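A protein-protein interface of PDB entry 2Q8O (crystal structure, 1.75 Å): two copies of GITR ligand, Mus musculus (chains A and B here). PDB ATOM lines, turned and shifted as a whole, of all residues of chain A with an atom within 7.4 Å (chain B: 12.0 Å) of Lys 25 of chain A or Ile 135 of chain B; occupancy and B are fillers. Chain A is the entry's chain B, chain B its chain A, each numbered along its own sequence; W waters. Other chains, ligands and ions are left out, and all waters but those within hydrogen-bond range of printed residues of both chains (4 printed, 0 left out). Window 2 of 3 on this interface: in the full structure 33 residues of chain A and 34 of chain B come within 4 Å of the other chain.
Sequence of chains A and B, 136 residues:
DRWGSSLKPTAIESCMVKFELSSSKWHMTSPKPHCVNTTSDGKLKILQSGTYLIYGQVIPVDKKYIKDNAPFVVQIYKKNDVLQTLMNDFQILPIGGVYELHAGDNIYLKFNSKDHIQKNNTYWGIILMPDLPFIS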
ATOM      1  N   LYS A  18      -9.628  18.583  11.817  1.00  0.00           N
ATOM      2  CA  LYS A  18      -8.767  19.144  12.851  1.00  0.00           C
ATOM      3  C   LYS A  18      -8.021  20.312  12.242  1.00  0.00           C
ATOM      4  O   LYS A  18      -7.234  20.136  11.291  1.00  0.00           O
ATOM      5  CB  LYS A  18      -7.760  18.089  13.330  1.00  0.00           C
ATOM      6  CG  LYS A  18      -6.870  18.567  14.498  1.00  0.00           C
ATOM      7  CD  LYS A  18      -5.876  17.480  14.942  1.00  0.00           C
ATOM      8  CE  LYS A  18      -4.849  17.197  13.884  1.00  0.00           C
ATOM      9  NZ  LYS A  18      -3.638  16.548  14.475  1.00  0.00           N
ATOM     10  N   PHE A  19      -8.251  21.498  12.800  1.00  0.00           N
ATOM     11  CA  PHE A  19      -7.564  22.688  12.352  1.00  0.00           C
ATOM     12  C   PHE A  19      -6.326  22.903  13.198  1.00  0.00           C
ATOM     13  O   PHE A  19      -6.420  23.013  14.422  1.00  0.00           O
ATOM     14  CB  PHE A  19      -8.504  23.878  12.484  1.00  0.00           C
ATOM     15  CG  PHE A  19      -7.956  25.169  11.935  1.00  0.00           C
ATOM     16  CD1 PHE A  19      -7.846  25.370  10.551  1.00  0.00           C
ATOM     17  CD2 PHE A  19      -7.559  26.175  12.801  1.00  0.00           C
ATOM     18  CE1 PHE A  19      -7.361  26.580  10.054  1.00  0.00           C
ATOM     19  CE2 PHE A  19      -7.051  27.396  12.299  1.00  0.00           C
ATOM     20  CZ  PHE A  19      -6.978  27.597  10.937  1.00  0.00           C
ATOM     21  N   GLU A  20      -5.173  23.000  12.544  1.00  0.00           N
ATOM     22  CA  GLU A  20      -3.929  23.299  13.246  1.00  0.00           C
ATOM     23  C   GLU A  20      -3.632  24.797  13.104  1.00  0.00           C
ATOM     24  O   GLU A  20      -3.377  25.280  11.983  1.00  0.00           O
ATOM     25  CB  GLU A  20      -2.772  22.469  12.671  1.00  0.00           C
ATOM     26  CG  GLU A  20      -2.914  20.963  12.859  1.00  0.00           C
ATOM     27  CD  GLU A  20      -2.496  20.459  14.239  1.00  0.00           C
ATOM     28  OE1 GLU A  20      -2.109  21.256  15.131  1.00  0.00           O
ATOM     29  OE2 GLU A  20      -2.548  19.228  14.433  1.00  0.00           O
ATOM     30  N   LEU A  21      -3.677  25.524  14.221  1.00  0.00           N
ATOM     31  CA  LEU A  21      -3.409  26.968  14.192  1.00  0.00           C
ATOM     32  C   LEU A  21      -1.984  27.304  13.719  1.00  0.00           C
ATOM     33  O   LEU A  21      -1.746  28.386  13.197  1.00  0.00           O
ATOM     34  CB  LEU A  21      -3.689  27.605  15.560  1.00  0.00           C
ATOM     35  CG  LEU A  21      -4.716  28.742  15.640  1.00  0.00           C
ATOM     36  CD1 LEU A  21      -4.405  29.674  16.821  1.00  0.00           C
ATOM     37  CD2 LEU A  21      -4.846  29.532  14.322  1.00  0.00           C
ATOM     38  N   SER A  22      -1.054  26.366  13.887  1.00  0.00           N
ATOM     39  CA  SER A  22       0.358  26.576  13.501  1.00  0.00           C
ATOM     40  C   SER A  22       0.480  26.835  11.993  1.00  0.00           C
ATOM     41  O   SER A  22       1.245  27.703  11.561  1.00  0.00           O
ATOM     42  CB  SER A  22       1.220  25.375  13.914  1.00  0.00           C
ATOM     43  OG  SER A  22       0.816  24.176  13.272  1.00  0.00           O
ATOM     44  N   SER A  23      -0.321  26.118  11.207  1.00  0.00           N
ATOM     45  CA  SER A  23      -0.211  26.150   9.746  1.00  0.00           C
ATOM     46  C   SER A  23      -1.451  26.745   9.094  1.00  0.00           C
ATOM     47  O   SER A  23      -1.454  26.985   7.891  1.00  0.00           O
ATOM     48  CB  SER A  23      -0.048  24.723   9.211  1.00  0.00           C
ATOM     49  OG  SER A  23      -1.148  23.907   9.642  1.00  0.00           O
ATOM     50  N   SER A  24      -2.520  26.914   9.880  1.00  0.00           N
ATOM     51  CA  SER A  24      -3.854  27.271   9.363  1.00  0.00           C
ATOM     52  C   SER A  24      -4.375  26.282   8.318  1.00  0.00           C
ATOM     53  O   SER A  24      -5.047  26.662   7.352  1.00  0.00           O
ATOM     54  CB  SER A  24      -3.925  28.732   8.894  1.00  0.00           C
ATOM     55  OG  SER A  24      -3.659  29.576  10.005  1.00  0.00           O
ATOM     56  N   LYS A  25      -4.056  25.010   8.547  1.00  0.00           N
ATOM     57  CA  LYS A  25      -4.481  23.916   7.680  1.00  0.00           C
ATOM     58  C   LYS A  25      -5.440  22.988   8.440  1.00  0.00           C
ATOM     59  O   LYS A  25      -5.266  22.760   9.641  1.00  0.00           O
ATOM     60  CB  LYS A  25      -3.278  23.123   7.143  1.00  0.00           C
ATOM     61  CG  LYS A  25      -2.288  23.959   6.288  1.00  0.00           C
ATOM     62  CD  LYS A  25      -2.920  24.417   4.995  1.00  0.00           C
ATOM     63  CE  LYS A  25      -1.941  25.312   4.197  1.00  0.00           C
ATOM     64  NZ  LYS A  25      -2.612  25.983   3.058  1.00  0.00           N
ATOM     65  N   TRP A  26      -6.440  22.485   7.721  1.00  0.00           N
ATOM     66  CA  TRP A  26      -7.335  21.447   8.242  1.00  0.00           C
ATOM     67  C   TRP A  26      -6.858  20.076   7.813  1.00  0.00           C
ATOM     68  O   TRP A  26      -6.569  19.837   6.626  1.00  0.00           O
ATOM     69  CB  TRP A  26      -8.758  21.619   7.728  1.00  0.00           C
ATOM     70  CG  TRP A  26      -9.502  22.795   8.258  1.00  0.00           C
ATOM     71  CD1 TRP A  26      -9.568  24.068   7.706  1.00  0.00           C
ATOM     72  CD2 TRP A  26     -10.321  22.827   9.435  1.00  0.00           C
ATOM     73  NE1 TRP A  26     -10.372  24.866   8.487  1.00  0.00           N
ATOM     74  CE2 TRP A  26     -10.853  24.133   9.543  1.00  0.00           C
ATOM     75  CE3 TRP A  26     -10.647  21.879  10.417  1.00  0.00           C
ATOM     76  CZ2 TRP A  26     -11.706  24.515  10.600  1.00  0.00           C
ATOM     77  CZ3 TRP A  26     -11.488  22.254  11.451  1.00  0.00           C
ATOM     78  CH2 TRP A  26     -12.013  23.555  11.535  1.00  0.00           C
ATOM     79  N   HIS A  27      -6.810  19.167   8.780  1.00  0.00           N
ATOM     80  CA  HIS A  27      -6.512  17.759   8.538  1.00  0.00           C
ATOM     81  C   HIS A  27      -7.845  17.011   8.572  1.00  0.00           C
ATOM     82  O   HIS A  27      -8.676  17.221   9.470  1.00  0.00           O
ATOM     83  CB  HIS A  27      -5.527  17.279   9.598  1.00  0.00           C
ATOM     84  CG  HIS A  27      -4.207  17.983   9.511  1.00  0.00           C
ATOM     85  ND1 HIS A  27      -3.050  17.338   9.149  1.00  0.00           N
ATOM     86  CD2 HIS A  27      -3.880  19.289   9.675  1.00  0.00           C
ATOM     87  CE1 HIS A  27      -2.057  18.211   9.104  1.00  0.00           C
ATOM     88  NE2 HIS A  27      -2.538  19.406   9.400  1.00  0.00           N
ATOM     89  N   MET A  28      -8.063  16.167   7.576  1.00  0.00           N
ATOM     90  CA  MET A  28      -9.417  15.651   7.313  1.00  0.00           C
ATOM     91  C   MET A  28      -9.481  14.162   6.998  1.00  0.00           C
ATOM     92  O   MET A  28      -8.546  13.585   6.449  1.00  0.00           O
ATOM     93  CB  MET A  28     -10.012  16.385   6.102  1.00  0.00           C
ATOM     94  CG  MET A  28      -9.686  17.892   6.042  1.00  0.00           C
ATOM     95  SD  MET A  28     -10.392  18.590   4.515  1.00  0.00           S
ATOM     96  CE  MET A  28      -9.355  17.820   3.266  1.00  0.00           C
ATOM     97  N   THR A  29     -10.639  13.570   7.277  1.00  0.00           N
ATOM     98  CA  THR A  29     -10.866  12.147   7.013  1.00  0.00           C
ATOM     99  C   THR A  29     -10.934  11.797   5.517  1.00  0.00           C
ATOM    100  O   THR A  29     -10.638  10.659   5.117  1.00  0.00           O
ATOM    101  CB  THR A  29     -12.159  11.664   7.695  1.00  0.00           C
ATOM    102  OG1 THR A  29     -13.146  12.700   7.643  1.00  0.00           O
ATOM    103  CG2 THR A  29     -11.876  11.332   9.186  1.00  0.00           C
ATOM    104  N   SER A  30     -11.387  12.745   4.706  1.00  0.00           N
ATOM    105  CA  SER A  30     -11.561  12.493   3.278  1.00  0.00           C
ATOM    106  C   SER A  30     -11.252  13.791   2.538  1.00  0.00           C
ATOM    107  O   SER A  30     -11.163  14.844   3.173  1.00  0.00           O
ATOM    108  CB  SER A  30     -12.985  11.997   2.971  1.00  0.00           C
ATOM    109  OG  SER A  30     -13.922  12.996   3.256  1.00  0.00           O
ATOM    110  N   PRO A  31     -11.065  13.723   1.201  1.00  0.00           N
ATOM    111  CA  PRO A  31     -10.800  14.965   0.459  1.00  0.00           C
ATOM    112  C   PRO A  31     -11.872  16.033   0.620  1.00  0.00           C
ATOM    113  O   PRO A  31     -11.545  17.214   0.674  1.00  0.00           O
ATOM    114  CB  PRO A  31     -10.712  14.505  -1.005  1.00  0.00           C
ATOM    115  CG  PRO A  31     -10.309  13.072  -0.924  1.00  0.00           C
ATOM    116  CD  PRO A  31     -10.985  12.540   0.333  1.00  0.00           C
ATOM    117  N   THR A  39     -13.004  26.362   6.342  1.00  0.00           N
ATOM    118  CA  THR A  39     -12.356  27.475   5.653  1.00  0.00           C
ATOM    119  C   THR A  39     -11.022  27.837   6.318  1.00  0.00           C
ATOM    120  O   THR A  39     -10.755  27.462   7.448  1.00  0.00           O
ATOM    121  CB  THR A  39     -13.310  28.699   5.500  1.00  0.00           C
ATOM    122  OG1 THR A  39     -14.045  28.901   6.713  1.00  0.00           O
ATOM    123  CG2 THR A  39     -14.323  28.469   4.372  1.00  0.00           C
ATOM    124  N   SER A  40     -10.180  28.560   5.586  1.00  0.00           N
ATOM    125  CA  SER A  40      -8.781  28.726   5.974  1.00  0.00           C
ATOM    126  C   SER A  40      -8.622  29.668   7.157  1.00  0.00           C
ATOM    127  O   SER A  40      -7.533  29.791   7.720  1.00  0.00           O
ATOM    128  CB  SER A  40      -7.977  29.232   4.779  1.00  0.00           C
ATOM    129  OG  SER A  40      -8.442  30.517   4.431  1.00  0.00           O
ATOM    130  N   TRP A 124      -8.233  22.755  16.964  1.00  0.00           N
ATOM    131  CA  TRP A 124      -9.623  22.478  17.283  1.00  0.00           C
ATOM    132  C   TRP A 124     -10.299  21.846  16.103  1.00  0.00           C
ATOM    133  O   TRP A 124      -9.796  21.879  14.983  1.00  0.00           O
ATOM    134  CB  TRP A 124     -10.385  23.738  17.668  1.00  0.00           C
ATOM    135  CG  TRP A 124     -10.396  24.828  16.600  1.00  0.00           C
ATOM    136  CD1 TRP A 124     -11.224  24.925  15.534  1.00  0.00           C
ATOM    137  CD2 TRP A 124      -9.549  25.981  16.565  1.00  0.00           C
ATOM    138  NE1 TRP A 124     -10.951  26.068  14.817  1.00  0.00           N
ATOM    139  CE2 TRP A 124      -9.925  26.739  15.440  1.00  0.00           C
ATOM    140  CE3 TRP A 124      -8.505  26.448  17.391  1.00  0.00           C
ATOM    141  CZ2 TRP A 124      -9.294  27.957  15.102  1.00  0.00           C
ATOM    142  CZ3 TRP A 124      -7.868  27.655  17.055  1.00  0.00           C
ATOM    143  CH2 TRP A 124      -8.276  28.398  15.926  1.00  0.00           C
ATOM    144  N   PRO B 130     -10.247   8.276  13.347  1.00  0.00           N
ATOM    145  CA  PRO B 130      -9.946   7.875  11.998  1.00  0.00           C
ATOM    146  C   PRO B 130      -8.646   8.575  11.587  1.00  0.00           C
ATOM    147  O   PRO B 130      -8.343   9.646  12.112  1.00  0.00           O
ATOM    148  CB  PRO B 130     -11.145   8.402  11.195  1.00  0.00           C
ATOM    149  CG  PRO B 130     -11.659   9.566  11.965  1.00  0.00           C
ATOM    150  CD  PRO B 130     -11.360   9.243  13.424  1.00  0.00           C
ATOM    151  N   ASP B 131      -7.897   7.973  10.669  1.00  0.00           N
ATOM    152  CA  ASP B 131      -6.745   8.647  10.053  1.00  0.00           C
ATOM    153  C   ASP B 131      -7.213   9.953   9.415  1.00  0.00           C
ATOM    154  O   ASP B 131      -8.340  10.017   8.900  1.00  0.00           O
ATOM    155  CB  ASP B 131      -6.112   7.762   8.980  1.00  0.00           C
ATOM    156  CG  ASP B 131      -5.529   6.463   9.534  1.00  0.00           C
ATOM    157  OD1 ASP B 131      -5.452   6.296  10.769  1.00  0.00           O
ATOM    158  OD2 ASP B 131      -5.144   5.599   8.717  1.00  0.00           O
ATOM    159  N   LEU B 132      -6.346  10.978   9.433  1.00  0.00           N
ATOM    160  CA  LEU B 132      -6.666  12.280   8.846  1.00  0.00           C
ATOM    161  C   LEU B 132      -5.646  12.634   7.760  1.00  0.00           C
ATOM    162  O   LEU B 132      -4.927  13.614   7.885  1.00  0.00           O
ATOM    163  CB  LEU B 132      -6.671  13.375   9.908  1.00  0.00           C
ATOM    164  CG  LEU B 132      -7.569  13.166  11.138  1.00  0.00           C
ATOM    165  CD1 LEU B 132      -7.376  14.370  12.054  1.00  0.00           C
ATOM    166  CD2 LEU B 132      -9.022  13.064  10.732  1.00  0.00           C
ATOM    167  N   PRO B 133      -5.630  11.863   6.672  1.00  0.00           N
ATOM    168  CA  PRO B 133      -4.520  11.998   5.714  1.00  0.00           C
ATOM    169  C   PRO B 133      -4.623  13.218   4.793  1.00  0.00           C
ATOM    170  O   PRO B 133      -3.613  13.622   4.189  1.00  0.00           O
ATOM    171  CB  PRO B 133      -4.601  10.712   4.908  1.00  0.00           C
ATOM    172  CG  PRO B 133      -6.072  10.318   4.972  1.00  0.00           C
ATOM    173  CD  PRO B 133      -6.610  10.834   6.271  1.00  0.00           C
ATOM    174  N   PHE B 134      -5.817  13.788   4.653  1.00  0.00           N
ATOM    175  CA  PHE B 134      -5.999  14.844   3.676  1.00  0.00           C
ATOM    176  C   PHE B 134      -5.920  16.187   4.358  1.00  0.00           C
ATOM    177  O   PHE B 134      -6.374  16.342   5.508  1.00  0.00           O
ATOM    178  CB  PHE B 134      -7.304  14.677   2.940  1.00  0.00           C
ATOM    179  CG  PHE B 134      -7.390  13.363   2.226  1.00  0.00           C
ATOM    180  CD1 PHE B 134      -8.093  12.303   2.789  1.00  0.00           C
ATOM    181  CD2 PHE B 134      -6.710  13.163   1.019  1.00  0.00           C
ATOM    182  CE1 PHE B 134      -8.152  11.059   2.138  1.00  0.00           C
ATOM    183  CE2 PHE B 134      -6.783  11.937   0.364  1.00  0.00           C
ATOM    184  CZ  PHE B 134      -7.508  10.885   0.928  1.00  0.00           C
ATOM    185  N   ILE B 135      -5.327  17.153   3.666  1.00  0.00           N
ATOM    186  CA  ILE B 135      -5.058  18.460   4.280  1.00  0.00           C
ATOM    187  C   ILE B 135      -5.549  19.545   3.345  1.00  0.00           C
ATOM    188  O   ILE B 135      -5.324  19.467   2.132  1.00  0.00           O
ATOM    189  CB  ILE B 135      -3.527  18.631   4.549  1.00  0.00           C
ATOM    190  CG1 ILE B 135      -2.992  17.477   5.415  1.00  0.00           C
ATOM    191  CG2 ILE B 135      -3.228  20.027   5.117  1.00  0.00           C
ATOM    192  CD1 ILE B 135      -1.454  17.359   5.463  1.00  0.00           C
ATOM    193  N   SER B 136      -6.236  20.552   3.875  1.00  0.00           N
ATOM    194  CA  SER B 136      -6.699  21.644   3.022  1.00  0.00           C
ATOM    195  C   SER B 136      -6.547  23.009   3.688  1.00  0.00           C
ATOM    196  O   SER B 136      -6.581  24.061   3.024  1.00  0.00           O
ATOM    197  CB  SER B 136      -8.135  21.396   2.600  1.00  0.00           C
ATOM    198  OG  SER B 136      -8.943  21.287   3.770  1.00  0.00           O
ATOM    199  OXT SER B 136      -6.420  23.069   4.918  1.00  0.00           O
HETATM  200  O   HOH W   1      -5.318  26.919   3.350  1.00  0.00           O
HETATM  201  O   HOH W   2      -6.935  25.756   5.417  1.00  0.00           O
HETATM  202  O   HOH W   3      -2.636  14.606   8.849  1.00  0.00           O
HETATM  203  O   HOH W   4      -9.784   8.642   7.052  1.00  0.00           O
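O of Phe 134 of chain B lies within hydrogen-bond range of N of Met 28 of chain A.
N of Ser 136 of chain B is in hydrogen-bond range of O of Trp 26 of chain A.
SD of Met 28 of chain A is in hydrogen-bond range of OG of Ser 136 of chain B (3.2 Å).
The backbone nitrogen (N) of Pro 133 of chain B lies close to the backbone carbonyl oxygen (O) of Met 28 of chain A, at 3.4 Å.
The side-chain amino group of Lys 18 of chain A lies within salt-bridge range of the side-chain carboxylate of Glu 20 of chain A (2.9 Å).
O of Lys 18 of chain A lies within hydrogen-bond range of N of His 27 of chain A.
O of Lys 25 of chain A lies within hydrogen-bond range of N of Glu 20 of chain A, 2.9 Å away.
The side-chain hydroxyl (OG) of Ser 23 of chain A sits close to the backbone NH (N) of Lys 25 of chain A, at 3.3 Å.
NE1 of Trp 26 of chain A sits at hydrogen-bond distance from O of Thr 39 of chain A (2.8 Å).
Among the printed residues, merely in contact across the chains: Trp 26 of chain A with Ile 135 of chain B (3.1 Å), Thr 29 of chain A with Pro 130 of chain B (3.3 Å), Met 28 of chain A with Leu 132 of chain B (3.3 Å), His 27 of chain A with Phe 134 of chain B (3.3 Å), Lys 25 of chain A with Ser 136 of chain B (3.5 Å), Ser 30 of chain A with Phe 134 of chain B (3.5 Å), Pro 31 of chain A with Phe 134 of chain B (3.7 Å), Trp 26 of chain A with Phe 134 of chain B (3.7 Å), Thr 29 of chain A with Leu 132 of chain B (3.7 Å), Lys 25 of chain A with Ile 135 of chain B (3.7 Å), His 27 of chain A with Ile 135 of chain B (3.7 Å), Thr 29 of chain A with Asp 131 of chain B (3.8 Å), Thr 29 of chain A with Phe 134 of chain B (3.8 Å) and Lys 18 of chain A with Leu 132 of chain B (3.95 Å).
Ile 135 of chain B touches just these residues of chain A: Lys 25, Trp 26 and His 27.
No residue of chain B comes within 4 Å of Phe 19 of chain A.
No residue of chain B comes within 4 Å of Glu 20 of chain A.
No residue of chain B comes within 4 Å of Ser 22 of chain A.
Ser 23 of chain A touches none of the printed residues of chain B.
No residue of chain B comes within 4 Å of Ser 24 of chain A.
Trp 26 of chain A touches just these residues of chain B: Phe 134, Ile 135 and Ser 136.
His 27 of chain A touches two residues of chain B.
No residue of chain B comes within 4 Å of Ser 40 of chain A.
Printed residues of chain A within 4 Å of Phe 134 of chain B: Trp 26 (3.7 Å), His 27 (3.3 Å), Met 28 (2.7 Å), Thr 29 (3.8 Å), Ser 30 (3.5 Å) and Pro 31 (3.7 Å).
Of the printed residues of chain A, Pro 130 of chain B touches Thr 29.
Thr 39 of chain A touches none of the printed residues of chain B.
Trp 124 of chain A touches none of the printed residues of chain B.
The nearest residue of chain A that does not touch Ile 135 of chain B is Met 28 of chain A (4.1 Å).
Printed residues of chain B that touch a printed residue of chain A: Pro 130, Asp 131, Leu 132, Pro 133, Phe 134, Ile 135 and Ser 136.
Hydrophobic or aromatic side chains of chain B within 4 Å of the printed part of chain A: Pro 130, Leu 132, Pro 133, Phe 134 and Ile 135.
Of the 17 printed residues of chain A, 8 touch a printed residue of chain B.
Printed residues of chain A that touch a printed residue of chain B: Lys 18, Lys 25, Trp 26, His 27, Met 28, Thr 29, Ser 30 and Pro 31.
Hydrophobic or aromatic side chains of chain A that line the printed part of chain B: Trp 26, His 27, Met 28 and Pro 31.
Among the printed residues, no Asp or Glu carboxylate lies within 4 Å of a Lys or Arg side-chain nitrogen of the other chain.
No position is printed for both chains.
Of the 18 pairs that touch across the chains among the printed residues, none has its exchanged pair printed and touching as well.
Water W3 lies within hydrogen-bond range of O of Leu 132 of chain B and ND1 of His 27 of chain A.
Water W4 lies within hydrogen-bond range of the backbone carbonyl oxygen of Asp 131 of chain B (2.7 Å) and the backbone carbonyl oxygen of Thr 29 of chain A (2.9 Å).
Water W2 lies within hydrogen-bond range of the chain-end carboxylate (OXT) of Ser 136 of chain B and the backbone carbonyl oxygen (O) of Ser 24 of chain A.
Water W1 lies within hydrogen-bond range of the side-chain amino group of Lys 25 of chain A (2.9 Å) and the chain-end carboxylate of Ser 136 of chain B (3.1 Å).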
